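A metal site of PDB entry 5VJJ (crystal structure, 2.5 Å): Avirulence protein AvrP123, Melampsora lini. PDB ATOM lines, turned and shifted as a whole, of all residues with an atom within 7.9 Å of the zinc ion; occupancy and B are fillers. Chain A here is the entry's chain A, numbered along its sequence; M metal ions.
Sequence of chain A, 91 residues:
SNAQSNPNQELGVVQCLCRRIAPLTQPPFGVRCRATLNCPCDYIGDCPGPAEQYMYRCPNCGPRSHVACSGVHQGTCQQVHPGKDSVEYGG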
ATOM      1  N   VAL A  31      20.264  -1.334  30.845  1.00  0.00           N
ATOM      2  CA  VAL A  31      20.036   0.085  30.617  1.00  0.00           C
ATOM      3  C   VAL A  31      19.164   0.254  29.378  1.00  0.00           C
ATOM      4  O   VAL A  31      18.963  -0.685  28.601  1.00  0.00           O
ATOM      5  CB  VAL A  31      21.344   0.885  30.442  1.00  0.00           C
ATOM      6  CG1 VAL A  31      22.059   1.032  31.761  1.00  0.00           C
ATOM      7  CG2 VAL A  31      22.249   0.225  29.409  1.00  0.00           C
ATOM      8  N   ARG A  32      18.646   1.462  29.190  1.00  0.00           N
ATOM      9  CA  ARG A  32      17.944   1.810  27.962  1.00  0.00           C
ATOM     10  C   ARG A  32      18.943   1.899  26.819  1.00  0.00           C
ATOM     11  O   ARG A  32      20.001   2.520  26.951  1.00  0.00           O
ATOM     12  CB  ARG A  32      17.219   3.140  28.119  1.00  0.00           C
ATOM     13  CG  ARG A  32      15.997   3.127  29.007  1.00  0.00           C
ATOM     14  CD  ARG A  32      15.373   4.526  29.084  1.00  0.00           C
ATOM     15  NE  ARG A  32      14.129   4.538  29.829  1.00  0.00           N
ATOM     16  CZ  ARG A  32      13.476   5.647  30.183  1.00  0.00           C
ATOM     17  NH1 ARG A  32      13.955   6.832  29.856  1.00  0.00           N
ATOM     18  NH2 ARG A  32      12.338   5.564  30.854  1.00  0.00           N
ATOM     19  N   CYS A  33      18.596   1.299  25.679  1.00  0.00           N
ATOM     20  CA  CYS A  33      19.372   1.445  24.461  1.00  0.00           C
ATOM     21  C   CYS A  33      18.931   2.704  23.735  1.00  0.00           C
ATOM     22  O   CYS A  33      17.733   2.870  23.449  1.00  0.00           O
ATOM     23  CB  CYS A  33      19.221   0.211  23.561  1.00  0.00           C
ATOM     24  SG  CYS A  33      20.109   0.399  22.005  1.00  0.00           S
ATOM     25  N   ARG A  34      19.880   3.579  23.431  1.00  0.00           N
ATOM     26  CA  ARG A  34      19.601   4.867  22.805  1.00  0.00           C
ATOM     27  C   ARG A  34      19.840   4.871  21.295  1.00  0.00           C
ATOM     28  O   ARG A  34      19.693   5.924  20.668  1.00  0.00           O
ATOM     29  CB  ARG A  34      20.444   5.964  23.462  1.00  0.00           C
ATOM     30  CG  ARG A  34      20.058   6.254  24.898  1.00  0.00           C
ATOM     31  CD  ARG A  34      20.930   7.340  25.489  1.00  0.00           C
ATOM     32  NE  ARG A  34      20.207   8.117  26.487  1.00  0.00           N
ATOM     33  CZ  ARG A  34      20.707   9.187  27.113  1.00  0.00           C
ATOM     34  NH1 ARG A  34      21.940   9.599  26.849  1.00  0.00           N
ATOM     35  NH2 ARG A  34      19.968   9.833  28.005  1.00  0.00           N
ATOM     36  N   ALA A  35      20.195   3.728  20.714  1.00  0.00           N
ATOM     37  CA  ALA A  35      20.445   3.687  19.281  1.00  0.00           C
ATOM     38  C   ALA A  35      19.186   4.016  18.495  1.00  0.00           C
ATOM     39  O   ALA A  35      18.060   3.791  18.957  1.00  0.00           O
ATOM     40  CB  ALA A  35      20.961   2.305  18.871  1.00  0.00           C
ATOM     41  N   THR A  36      19.372   4.588  17.311  1.00  0.00           N
ATOM     42  CA  THR A  36      18.277   4.805  16.364  1.00  0.00           C
ATOM     43  C   THR A  36      18.179   3.639  15.400  1.00  0.00           C
ATOM     44  O   THR A  36      19.183   3.015  15.054  1.00  0.00           O
ATOM     45  CB  THR A  36      18.479   6.100  15.571  1.00  0.00           C
ATOM     46  OG1 THR A  36      19.789   6.109  14.987  1.00  0.00           O
ATOM     47  CG2 THR A  36      18.308   7.325  16.462  1.00  0.00           C
ATOM     48  N   LEU A  37      16.965   3.355  14.963  1.00  0.00           N
ATOM     49  CA  LEU A  37      16.687   2.196  14.115  1.00  0.00           C
ATOM     50  C   LEU A  37      16.657   2.601  12.652  1.00  0.00           C
ATOM     51  O   LEU A  37      16.266   3.716  12.290  1.00  0.00           O
ATOM     52  CB  LEU A  37      15.359   1.556  14.510  1.00  0.00           C
ATOM     53  CG  LEU A  37      15.188   1.285  16.011  1.00  0.00           C
ATOM     54  CD1 LEU A  37      13.778   0.785  16.296  1.00  0.00           C
ATOM     55  CD2 LEU A  37      16.228   0.298  16.526  1.00  0.00           C
ATOM     56  N   ASP A  46      12.022   3.061  19.735  1.00  0.00           N
ATOM     57  CA  ASP A  46      13.185   2.760  20.562  1.00  0.00           C
ATOM     58  C   ASP A  46      13.535   1.287  20.471  1.00  0.00           C
ATOM     59  O   ASP A  46      12.659   0.415  20.333  1.00  0.00           O
ATOM     60  CB  ASP A  46      12.910   3.115  22.022  1.00  0.00           C
ATOM     61  CG  ASP A  46      12.335   4.507  22.184  1.00  0.00           C
ATOM     62  OD1 ASP A  46      12.770   5.429  21.460  1.00  0.00           O
ATOM     63  OD2 ASP A  46      11.462   4.676  23.060  1.00  0.00           O
ATOM     64  N   CYS A  47      14.822   0.994  20.560  1.00  0.00           N
ATOM     65  CA  CYS A  47      15.258  -0.389  20.674  1.00  0.00           C
ATOM     66  C   CYS A  47      14.846  -0.946  22.022  1.00  0.00           C
ATOM     67  O   CYS A  47      15.174  -0.355  23.062  1.00  0.00           O
ATOM     68  CB  CYS A  47      16.777  -0.486  20.512  1.00  0.00           C
ATOM     69  SG  CYS A  47      17.399  -2.151  20.854  1.00  0.00           S
ATOM     70  N   PRO A  48      14.128  -2.087  22.069  1.00  0.00           N
ATOM     71  CA  PRO A  48      13.761  -2.677  23.369  1.00  0.00           C
ATOM     72  C   PRO A  48      14.914  -3.359  24.094  1.00  0.00           C
ATOM     73  O   PRO A  48      14.688  -3.887  25.190  1.00  0.00           O
ATOM     74  CB  PRO A  48      12.691  -3.709  22.994  1.00  0.00           C
ATOM     75  CG  PRO A  48      12.289  -3.389  21.591  1.00  0.00           C
ATOM     76  CD  PRO A  48      13.477  -2.790  20.954  1.00  0.00           C
ATOM     77  N   GLY A  49      16.116  -3.369  23.537  1.00  0.00           N
ATOM     78  CA  GLY A  49      17.228  -4.082  24.153  1.00  0.00           C
ATOM     79  C   GLY A  49      17.290  -5.525  23.683  1.00  0.00           C
ATOM     80  O   GLY A  49      16.707  -5.872  22.647  1.00  0.00           O
ATOM     81  N   PRO A  50      17.983  -6.393  24.437  1.00  0.00           N
ATOM     82  CA  PRO A  50      18.642  -6.102  25.717  1.00  0.00           C
ATOM     83  C   PRO A  50      19.946  -5.314  25.583  1.00  0.00           C
ATOM     84  O   PRO A  50      20.781  -5.619  24.716  1.00  0.00           O
ATOM     85  CB  PRO A  50      18.929  -7.502  26.297  1.00  0.00           C
ATOM     86  CG  PRO A  50      18.201  -8.479  25.406  1.00  0.00           C
ATOM     87  CD  PRO A  50      18.096  -7.809  24.084  1.00  0.00           C
ATOM     88  N   ALA A  51      20.126  -4.312  26.449  1.00  0.00           N
ATOM     89  CA  ALA A  51      21.336  -3.515  26.478  1.00  0.00           C
ATOM     90  C   ALA A  51      21.893  -3.498  27.897  1.00  0.00           C
ATOM     91  O   ALA A  51      21.150  -3.534  28.876  1.00  0.00           O
ATOM     92  CB  ALA A  51      21.067  -2.078  26.006  1.00  0.00           C
ATOM     93  N   VAL A  67      28.177   1.126  26.582  1.00  0.00           N
ATOM     94  CA  VAL A  67      26.967   0.317  26.573  1.00  0.00           C
ATOM     95  C   VAL A  67      27.011  -0.619  25.365  1.00  0.00           C
ATOM     96  O   VAL A  67      27.510  -0.258  24.303  1.00  0.00           O
ATOM     97  CB  VAL A  67      25.698   1.204  26.536  1.00  0.00           C
ATOM     98  CG1 VAL A  67      24.439   0.360  26.356  1.00  0.00           C
ATOM     99  CG2 VAL A  67      25.595   2.019  27.821  1.00  0.00           C
ATOM    100  N   ALA A  68      26.481  -1.826  25.562  1.00  0.00           N
ATOM    101  CA  ALA A  68      26.373  -2.823  24.505  1.00  0.00           C
ATOM    102  C   ALA A  68      24.945  -3.346  24.457  1.00  0.00           C
ATOM    103  O   ALA A  68      24.278  -3.441  25.487  1.00  0.00           O
ATOM    104  CB  ALA A  68      27.349  -3.996  24.731  1.00  0.00           C
ATOM    105  N   CYS A  69      24.486  -3.663  23.251  1.00  0.00           N
ATOM    106  CA  CYS A  69      23.094  -4.035  23.028  1.00  0.00           C
ATOM    107  C   CYS A  69      23.016  -5.177  22.037  1.00  0.00           C
ATOM    108  O   CYS A  69      23.723  -5.171  21.023  1.00  0.00           O
ATOM    109  CB  CYS A  69      22.263  -2.851  22.518  1.00  0.00           C
ATOM    110  SG  CYS A  69      20.493  -3.189  22.374  1.00  0.00           S
ATOM    111  N   SER A  70      22.141  -6.148  22.314  1.00  0.00           N
ATOM    112  CA  SER A  70      21.917  -7.282  21.427  1.00  0.00           C
ATOM    113  C   SER A  70      20.673  -7.127  20.572  1.00  0.00           C
ATOM    114  O   SER A  70      20.394  -7.998  19.739  1.00  0.00           O
ATOM    115  CB  SER A  70      21.813  -8.568  22.255  1.00  0.00           C
ATOM    116  OG  SER A  70      23.056  -8.890  22.849  1.00  0.00           O
ATOM    117  N   GLY A  71      19.909  -6.052  20.741  1.00  0.00           N
ATOM    118  CA  GLY A  71      18.769  -5.798  19.888  1.00  0.00           C
ATOM    119  C   GLY A  71      19.182  -5.594  18.439  1.00  0.00           C
ATOM    120  O   GLY A  71      20.355  -5.396  18.109  1.00  0.00           O
ATOM    121  N   VAL A  72      18.189  -5.634  17.564  1.00  0.00           N
ATOM    122  CA  VAL A  72      18.399  -5.427  16.138  1.00  0.00           C
ATOM    123  C   VAL A  72      18.196  -3.948  15.841  1.00  0.00           C
ATOM    124  O   VAL A  72      17.099  -3.421  16.031  1.00  0.00           O
ATOM    125  CB  VAL A  72      17.459  -6.301  15.297  1.00  0.00           C
ATOM    126  CG1 VAL A  72      17.689  -6.055  13.810  1.00  0.00           C
ATOM    127  CG2 VAL A  72      17.665  -7.776  15.618  1.00  0.00           C
ATOM    128  N   HIS A  73      19.256  -3.280  15.379  1.00  0.00           N
ATOM    129  CA  HIS A  73      19.195  -1.866  15.043  1.00  0.00           C
ATOM    130  C   HIS A  73      19.035  -1.619  13.550  1.00  0.00           C
ATOM    131  O   HIS A  73      18.422  -0.602  13.172  1.00  0.00           O
ATOM    132  CB  HIS A  73      20.461  -1.163  15.531  1.00  0.00           C
ATOM    133  CG  HIS A  73      20.654  -1.228  17.012  1.00  0.00           C
ATOM    134  ND1 HIS A  73      21.818  -0.827  17.632  1.00  0.00           N
ATOM    135  CD2 HIS A  73      19.837  -1.660  18.004  1.00  0.00           C
ATOM    136  CE1 HIS A  73      21.696  -1.001  18.945  1.00  0.00           C
ATOM    137  NE2 HIS A  73      20.502  -1.502  19.187  1.00  0.00           N
HETATM  138 ZN    ZN M   1      19.681  -1.638  21.046  1.00  0.00          ZN
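The side-chain sulfur (SG) of Cys 69 lies close to the backbone NH (N) of Gly 71, at 3.3 Å.
N of Gly 49 sits close to SG of Cys 47.
The backbone carbonyl oxygen (O) of Pro 50 sits close to the side-chain sulfur (SG) of Cys 69, 3.4 Å away.
The backbone NH of Ala 35 sits close to the side-chain sulfur of Cys 33 (3.6 Å).
The zinc ion is bound by a ring nitrogen (NE2) of His 73 (2.0 Å), the side-chain sulfur of Cys 69 (2.2 Å), the side-chain sulfur of Cys 33 (2.3 Å) and the side-chain sulfur of Cys 47 (2.3 Å).
The zinc ion has four donor atoms within binding distance.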
